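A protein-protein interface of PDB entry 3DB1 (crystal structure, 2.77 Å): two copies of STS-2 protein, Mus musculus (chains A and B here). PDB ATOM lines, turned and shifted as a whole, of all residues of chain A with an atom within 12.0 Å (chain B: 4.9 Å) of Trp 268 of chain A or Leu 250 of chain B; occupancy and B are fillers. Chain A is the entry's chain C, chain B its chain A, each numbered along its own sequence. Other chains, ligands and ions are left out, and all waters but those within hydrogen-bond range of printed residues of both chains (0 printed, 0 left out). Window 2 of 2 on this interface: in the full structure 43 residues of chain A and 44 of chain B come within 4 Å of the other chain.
N of Val 251 of chain B sits at hydrogen-bond distance from O of Phe 238 of chain B (2.9 Å). The side-chain amide oxygen of Asn 267 of chain A sits close to the indole nitrogen of Trp 268 of chain A (3.4 Å).
Among the printed residues, merely in contact across the chains: Trp 268 of chain A with Asn 252 of chain B (3.1 Å), Trp 268 of chain A with Pro 253 of chain B (3.4 Å), Trp 268 of chain A with Val 251 of chain B (3.7 Å), Phe 266 of chain A with Met 236 of chain B (3.7 Å), Trp 268 of chain A with Leu 250 of chain B (3.8 Å) and Trp 271 of chain A with Cys 237 of chain B (3.9 Å).
Of the printed residues of chain B, Phe 266 of chain A touches Met 236 (3.7 Å). Of chain B, only Leu 250, Val 251, Asn 252 and Pro 253 come within 4 Å of Trp 268 of chain A. Printed residues of chain B within 4 Å of Trp 271 of chain A: Cys 237 (3.9 Å). Of the printed residues of chain A, Met 236 of chain B touches Phe 266. Of chain A, only Trp 271 comes within 4 Å of Cys 237 of chain B. No residue of chain A comes within 4 Å of Cys 239 of chain B. Of chain A, only Trp 268 comes within 4 Å of Leu 250 of chain B. Asn 252 of chain B touches one residue of chain A. Printed residues of chain A within 4 Å of Pro 253 of chain B: Trp 268 (3.4 Å). The nearest residue of chain B that does not touch Trp 268 of chain A is Met 236 of chain B (4.2 Å). The nearest residue of chain A that does not touch Leu 250 of chain B is Trp 271 of chain A (4.1 Å). The nearest printed residue of chain B that does not touch Trp 271 of chain A is Leu 250 of chain B (4.1 Å).
Of the 11 printed residues of chain A, 3 touch a printed residue of chain B. Hydrophobic or aromatic side chains of chain A that line the printed part of chain B: Phe 266, Trp 268 and Trp 271. Of the 11 printed residues of chain B, 6 touch a printed residue of chain A. Among the printed residues, 6 pairs touch across the chains.
No position is printed for both chains. Of the 6 pairs that touch across the chains among the printed residues, none has its exchanged pair printed and touching as well.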
ATOM      1  N   PRO A  43       8.390  -3.329 -33.974  1.00  0.00           N
ATOM      2  CA  PRO A  43       7.521  -2.465 -33.205  1.00  0.00           C
ATOM      3  C   PRO A  43       6.183  -3.109 -32.874  1.00  0.00           C
ATOM      4  O   PRO A  43       5.414  -2.539 -32.144  1.00  0.00           O
ATOM      5  CB  PRO A  43       7.309  -1.294 -34.145  1.00  0.00           C
ATOM      6  CG  PRO A  43       7.479  -1.848 -35.460  1.00  0.00           C
ATOM      7  CD  PRO A  43       8.458  -2.924 -35.384  1.00  0.00           C
ATOM      8  N   ASP A  44       5.920  -4.280 -33.445  1.00  0.00           N
ATOM      9  CA  ASP A  44       4.673  -4.992 -33.280  1.00  0.00           C
ATOM     10  C   ASP A  44       4.993  -6.421 -33.624  1.00  0.00           C
ATOM     11  O   ASP A  44       5.780  -6.670 -34.509  1.00  0.00           O
ATOM     12  CB  ASP A  44       3.599  -4.459 -34.229  1.00  0.00           C
ATOM     13  CG  ASP A  44       2.254  -5.195 -34.077  1.00  0.00           C
ATOM     14  OD1 ASP A  44       2.167  -6.412 -34.375  1.00  0.00           O
ATOM     15  OD2 ASP A  44       1.273  -4.540 -33.675  1.00  0.00           O
ATOM     16  N   SER A 264      -6.874  -6.121 -34.045  1.00  0.00           N
ATOM     17  CA  SER A 264      -6.635  -4.676 -34.160  1.00  0.00           C
ATOM     18  C   SER A 264      -5.649  -4.188 -33.115  1.00  0.00           C
ATOM     19  O   SER A 264      -5.479  -4.815 -32.093  1.00  0.00           O
ATOM     20  CB  SER A 264      -7.944  -3.891 -34.122  1.00  0.00           C
ATOM     21  OG  SER A 264      -8.655  -4.180 -32.944  1.00  0.00           O
ATOM     22  N   VAL A 265      -4.971  -3.089 -33.407  1.00  0.00           N
ATOM     23  CA  VAL A 265      -3.986  -2.532 -32.482  1.00  0.00           C
ATOM     24  C   VAL A 265      -4.625  -2.189 -31.128  1.00  0.00           C
ATOM     25  O   VAL A 265      -5.754  -1.689 -31.056  1.00  0.00           O
ATOM     26  CB  VAL A 265      -3.182  -1.308 -33.110  1.00  0.00           C
ATOM     27  CG1 VAL A 265      -4.075  -0.050 -33.325  1.00  0.00           C
ATOM     28  CG2 VAL A 265      -1.908  -0.979 -32.283  1.00  0.00           C
ATOM     29  N   PHE A 266      -3.894  -2.481 -30.061  1.00  0.00           N
ATOM     30  CA  PHE A 266      -4.364  -2.201 -28.705  1.00  0.00           C
ATOM     31  C   PHE A 266      -3.318  -1.422 -27.910  1.00  0.00           C
ATOM     32  O   PHE A 266      -2.131  -1.457 -28.230  1.00  0.00           O
ATOM     33  CB  PHE A 266      -4.720  -3.525 -28.014  1.00  0.00           C
ATOM     34  CG  PHE A 266      -5.156  -3.385 -26.580  1.00  0.00           C
ATOM     35  CD1 PHE A 266      -6.276  -2.616 -26.242  1.00  0.00           C
ATOM     36  CD2 PHE A 266      -4.454  -4.048 -25.564  1.00  0.00           C
ATOM     37  CE1 PHE A 266      -6.677  -2.486 -24.906  1.00  0.00           C
ATOM     38  CE2 PHE A 266      -4.843  -3.932 -24.242  1.00  0.00           C
ATOM     39  CZ  PHE A 266      -5.954  -3.145 -23.907  1.00  0.00           C
ATOM     40  N   ASN A 267      -3.769  -0.708 -26.888  1.00  0.00           N
ATOM     41  CA  ASN A 267      -2.874  -0.033 -25.957  1.00  0.00           C
ATOM     42  C   ASN A 267      -3.568   0.261 -24.628  1.00  0.00           C
ATOM     43  O   ASN A 267      -4.551   1.010 -24.552  1.00  0.00           O
ATOM     44  CB  ASN A 267      -2.265   1.225 -26.598  1.00  0.00           C
ATOM     45  CG  ASN A 267      -1.619   2.172 -25.587  1.00  0.00           C
ATOM     46  OD1 ASN A 267      -1.013   1.751 -24.594  1.00  0.00           O
ATOM     47  ND2 ASN A 267      -1.737   3.468 -25.856  1.00  0.00           N
ATOM     48  N   TRP A 268      -3.014  -0.377 -23.602  1.00  0.00           N
ATOM     49  CA  TRP A 268      -3.347  -0.216 -22.192  1.00  0.00           C
ATOM     50  C   TRP A 268      -3.372   1.241 -21.661  1.00  0.00           C
ATOM     51  O   TRP A 268      -3.899   1.478 -20.581  1.00  0.00           O
ATOM     52  CB  TRP A 268      -2.328  -1.039 -21.397  1.00  0.00           C
ATOM     53  CG  TRP A 268      -0.953  -0.478 -21.572  1.00  0.00           C
ATOM     54  CD1 TRP A 268      -0.121  -0.652 -22.640  1.00  0.00           C
ATOM     55  CD2 TRP A 268      -0.273   0.410 -20.672  1.00  0.00           C
ATOM     56  NE1 TRP A 268       1.042   0.057 -22.455  1.00  0.00           N
ATOM     57  CE2 TRP A 268       0.977   0.715 -21.255  1.00  0.00           C
ATOM     58  CE3 TRP A 268      -0.597   0.971 -19.420  1.00  0.00           C
ATOM     59  CZ2 TRP A 268       1.904   1.555 -20.634  1.00  0.00           C
ATOM     60  CZ3 TRP A 268       0.329   1.799 -18.798  1.00  0.00           C
ATOM     61  CH2 TRP A 268       1.567   2.080 -19.406  1.00  0.00           C
ATOM     62  N   ARG A 269      -2.780   2.192 -22.387  1.00  0.00           N
ATOM     63  CA  ARG A 269      -2.876   3.635 -22.056  1.00  0.00           C
ATOM     64  C   ARG A 269      -4.193   4.222 -22.569  1.00  0.00           C
ATOM     65  O   ARG A 269      -4.879   4.962 -21.860  1.00  0.00           O
ATOM     66  CB  ARG A 269      -1.688   4.432 -22.632  1.00  0.00           C
ATOM     67  CG  ARG A 269      -0.450   4.499 -21.734  1.00  0.00           C
ATOM     68  CD  ARG A 269      -0.643   5.473 -20.556  1.00  0.00           C
ATOM     69  NE  ARG A 269       0.085   5.050 -19.354  1.00  0.00           N
ATOM     70  CZ  ARG A 269       1.349   5.370 -19.067  1.00  0.00           C
ATOM     71  NH1 ARG A 269       2.074   6.137 -19.881  1.00  0.00           N
ATOM     72  NH2 ARG A 269       1.893   4.915 -17.951  1.00  0.00           N
ATOM     73  N   ASN A 270      -4.522   3.885 -23.815  1.00  0.00           N
ATOM     74  CA  ASN A 270      -5.833   4.121 -24.403  1.00  0.00           C
ATOM     75  C   ASN A 270      -6.923   3.319 -23.661  1.00  0.00           C
ATOM     76  O   ASN A 270      -7.805   2.713 -24.290  1.00  0.00           O
ATOM     77  CB  ASN A 270      -5.796   3.751 -25.898  1.00  0.00           C
ATOM     78  CG  ASN A 270      -6.831   4.506 -26.730  1.00  0.00           C
ATOM     79  OD1 ASN A 270      -7.356   5.541 -26.299  1.00  0.00           O
ATOM     80  ND2 ASN A 270      -7.120   3.992 -27.936  1.00  0.00           N
ATOM     81  N   TRP A 271      -6.822   3.291 -22.324  1.00  0.00           N
ATOM     82  CA  TRP A 271      -7.929   2.901 -21.447  1.00  0.00           C
ATOM     83  C   TRP A 271      -8.920   4.036 -21.626  1.00  0.00           C
ATOM     84  O   TRP A 271      -9.774   3.983 -22.519  1.00  0.00           O
ATOM     85  CB  TRP A 271      -7.512   2.821 -19.961  1.00  0.00           C
ATOM     86  CG  TRP A 271      -7.127   1.445 -19.336  1.00  0.00           C
ATOM     87  CD1 TRP A 271      -6.643   1.254 -18.062  1.00  0.00           C
ATOM     88  CD2 TRP A 271      -7.180   0.114 -19.939  1.00  0.00           C
ATOM     89  NE1 TRP A 271      -6.404  -0.088 -17.833  1.00  0.00           N
ATOM     90  CE2 TRP A 271      -6.720  -0.807 -18.959  1.00  0.00           C
ATOM     91  CE3 TRP A 271      -7.567  -0.384 -21.202  1.00  0.00           C
ATOM     92  CZ2 TRP A 271      -6.640  -2.188 -19.204  1.00  0.00           C
ATOM     93  CZ3 TRP A 271      -7.485  -1.759 -21.433  1.00  0.00           C
ATOM     94  CH2 TRP A 271      -7.024  -2.638 -20.440  1.00  0.00           C
ATOM     95  N   ILE A 272      -8.783   5.070 -20.790  1.00  0.00           N
ATOM     96  CA  ILE A 272      -9.465   6.343 -21.008  1.00  0.00           C
ATOM     97  C   ILE A 272      -8.668   7.083 -22.075  1.00  0.00           C
ATOM     98  O   ILE A 272      -9.245   7.628 -23.011  1.00  0.00           O
ATOM     99  CB  ILE A 272      -9.596   7.201 -19.713  1.00  0.00           C
ATOM    100  CG1 ILE A 272     -10.093   6.343 -18.529  1.00  0.00           C
ATOM    101  CG2 ILE A 272     -10.510   8.424 -19.970  1.00  0.00           C
ATOM    102  CD1 ILE A 272      -9.942   6.989 -17.127  1.00  0.00           C
ATOM    103  N   LEU B 214      -4.245  -2.104  -8.117  1.00  0.00           N
ATOM    104  CA  LEU B 214      -3.951  -0.682  -8.203  1.00  0.00           C
ATOM    105  C   LEU B 214      -4.654   0.134  -7.116  1.00  0.00           C
ATOM    106  O   LEU B 214      -4.503   1.345  -7.073  1.00  0.00           O
ATOM    107  CB  LEU B 214      -4.339  -0.138  -9.575  1.00  0.00           C
ATOM    108  CG  LEU B 214      -3.606  -0.733 -10.770  1.00  0.00           C
ATOM    109  CD1 LEU B 214      -4.271  -0.299 -12.048  1.00  0.00           C
ATOM    110  CD2 LEU B 214      -2.130  -0.364 -10.781  1.00  0.00           C
ATOM    111  N   MET B 236      -2.798  -7.518 -23.487  1.00  0.00           N
ATOM    112  CA  MET B 236      -2.150  -7.564 -22.174  1.00  0.00           C
ATOM    113  C   MET B 236      -2.221  -6.299 -21.359  1.00  0.00           C
ATOM    114  O   MET B 236      -2.272  -5.192 -21.888  1.00  0.00           O
ATOM    115  CB  MET B 236      -0.687  -7.862 -22.344  1.00  0.00           C
ATOM    116  CG  MET B 236      -0.459  -9.192 -22.800  1.00  0.00           C
ATOM    117  SD  MET B 236       1.242  -9.298 -23.159  1.00  0.00           S
ATOM    118  CE  MET B 236       1.263 -11.043 -23.681  1.00  0.00           C
ATOM    119  N   CYS B 237      -2.149  -6.497 -20.048  1.00  0.00           N
ATOM    120  CA  CYS B 237      -2.174  -5.422 -19.107  1.00  0.00           C
ATOM    121  C   CYS B 237      -1.168  -5.817 -18.017  1.00  0.00           C
ATOM    122  O   CYS B 237      -1.292  -6.885 -17.400  1.00  0.00           O
ATOM    123  CB  CYS B 237      -3.574  -5.362 -18.572  1.00  0.00           C
ATOM    124  SG  CYS B 237      -3.755  -4.100 -17.459  1.00  0.00           S
ATOM    125  N   PHE B 238      -0.160  -4.984 -17.798  1.00  0.00           N
ATOM    126  CA  PHE B 238       0.950  -5.323 -16.895  1.00  0.00           C
ATOM    127  C   PHE B 238       1.000  -4.495 -15.591  1.00  0.00           C
ATOM    128  O   PHE B 238       0.993  -3.255 -15.615  1.00  0.00           O
ATOM    129  CB  PHE B 238       2.251  -5.159 -17.664  1.00  0.00           C
ATOM    130  CG  PHE B 238       3.421  -5.767 -17.008  1.00  0.00           C
ATOM    131  CD1 PHE B 238       3.286  -6.917 -16.251  1.00  0.00           C
ATOM    132  CD2 PHE B 238       4.684  -5.232 -17.190  1.00  0.00           C
ATOM    133  CE1 PHE B 238       4.401  -7.520 -15.665  1.00  0.00           C
ATOM    134  CE2 PHE B 238       5.788  -5.816 -16.596  1.00  0.00           C
ATOM    135  CZ  PHE B 238       5.650  -6.963 -15.833  1.00  0.00           C
ATOM    136  N   CYS B 239       1.084  -5.173 -14.456  1.00  0.00           N
ATOM    137  CA  CYS B 239       1.250  -4.463 -13.182  1.00  0.00           C
ATOM    138  C   CYS B 239       2.537  -4.805 -12.467  1.00  0.00           C
ATOM    139  O   CYS B 239       2.905  -5.969 -12.406  1.00  0.00           O
ATOM    140  CB  CYS B 239       0.084  -4.758 -12.281  1.00  0.00           C
ATOM    141  SG  CYS B 239      -1.375  -3.961 -12.896  1.00  0.00           S
ATOM    142  N   TRP B 248       0.922  -1.071  -6.230  1.00  0.00           N
ATOM    143  CA  TRP B 248       1.095  -1.606  -7.569  1.00  0.00           C
ATOM    144  C   TRP B 248       0.973  -0.536  -8.633  1.00  0.00           C
ATOM    145  O   TRP B 248       0.108   0.310  -8.554  1.00  0.00           O
ATOM    146  CB  TRP B 248       0.082  -2.704  -7.841  1.00  0.00           C
ATOM    147  CG  TRP B 248       0.327  -3.918  -7.052  1.00  0.00           C
ATOM    148  CD1 TRP B 248      -0.069  -4.149  -5.768  1.00  0.00           C
ATOM    149  CD2 TRP B 248       1.013  -5.098  -7.487  1.00  0.00           C
ATOM    150  NE1 TRP B 248       0.328  -5.404  -5.377  1.00  0.00           N
ATOM    151  CE2 TRP B 248       1.000  -6.004  -6.408  1.00  0.00           C
ATOM    152  CE3 TRP B 248       1.636  -5.476  -8.682  1.00  0.00           C
ATOM    153  CZ2 TRP B 248       1.587  -7.257  -6.483  1.00  0.00           C
ATOM    154  CZ3 TRP B 248       2.211  -6.721  -8.758  1.00  0.00           C
ATOM    155  CH2 TRP B 248       2.181  -7.601  -7.667  1.00  0.00           C
ATOM    156  N   ASP B 249       1.835  -0.600  -9.640  1.00  0.00           N
ATOM    157  CA  ASP B 249       1.816   0.375 -10.720  1.00  0.00           C
ATOM    158  C   ASP B 249       1.516  -0.257 -12.076  1.00  0.00           C
ATOM    159  O   ASP B 249       2.069  -1.290 -12.447  1.00  0.00           O
ATOM    160  CB  ASP B 249       3.138   1.148 -10.770  1.00  0.00           C
ATOM    161  CG  ASP B 249       3.312   2.059  -9.588  1.00  0.00           C
ATOM    162  OD1 ASP B 249       2.472   2.970  -9.444  1.00  0.00           O
ATOM    163  OD2 ASP B 249       4.267   1.860  -8.794  1.00  0.00           O
ATOM    164  N   LEU B 250       0.638   0.403 -12.811  1.00  0.00           N
ATOM    165  CA  LEU B 250       0.302   0.000 -14.150  1.00  0.00           C
ATOM    166  C   LEU B 250       1.416   0.408 -15.117  1.00  0.00           C
ATOM    167  O   LEU B 250       1.707   1.586 -15.246  1.00  0.00           O
ATOM    168  CB  LEU B 250      -1.016   0.653 -14.537  1.00  0.00           C
ATOM    169  CG  LEU B 250      -1.659   0.142 -15.803  1.00  0.00           C
ATOM    170  CD1 LEU B 250      -2.045  -1.298 -15.618  1.00  0.00           C
ATOM    171  CD2 LEU B 250      -2.870   0.980 -16.094  1.00  0.00           C
ATOM    172  N   VAL B 251       2.055  -0.551 -15.783  1.00  0.00           N
ATOM    173  CA  VAL B 251       3.162  -0.232 -16.687  1.00  0.00           C
ATOM    174  C   VAL B 251       3.083  -0.939 -18.022  1.00  0.00           C
ATOM    175  O   VAL B 251       2.237  -1.822 -18.222  1.00  0.00           O
ATOM    176  CB  VAL B 251       4.536  -0.529 -16.060  1.00  0.00           C
ATOM    177  CG1 VAL B 251       4.771   0.388 -14.862  1.00  0.00           C
ATOM    178  CG2 VAL B 251       4.657  -1.974 -15.670  1.00  0.00           C
ATOM    179  N   ASN B 252       3.967  -0.550 -18.939  1.00  0.00           N
ATOM    180  CA  ASN B 252       4.034  -1.148 -20.278  1.00  0.00           C
ATOM    181  C   ASN B 252       4.284  -2.648 -20.236  1.00  0.00           C
ATOM    182  O   ASN B 252       5.157  -3.097 -19.503  1.00  0.00           O
ATOM    183  CB  ASN B 252       5.148  -0.538 -21.109  1.00  0.00           C
ATOM    184  CG  ASN B 252       5.075   0.962 -21.165  1.00  0.00           C
ATOM    185  OD1 ASN B 252       4.576   1.514 -22.145  1.00  0.00           O
ATOM    186  ND2 ASN B 252       5.570   1.654 -20.101  1.00  0.00           N
ATOM    187  N   PRO B 253       3.509  -3.421 -21.016  1.00  0.00           N
ATOM    188  CA  PRO B 253       3.716  -4.848 -21.064  1.00  0.00           C
ATOM    189  C   PRO B 253       5.062  -5.127 -21.683  1.00  0.00           C
ATOM    190  O   PRO B 253       5.563  -4.340 -22.510  1.00  0.00           O
ATOM    191  CB  PRO B 253       2.565  -5.350 -21.962  1.00  0.00           C
ATOM    192  CG  PRO B 253       1.535  -4.303 -21.892  1.00  0.00           C
ATOM    193  CD  PRO B 253       2.373  -3.030 -21.869  1.00  0.00           C
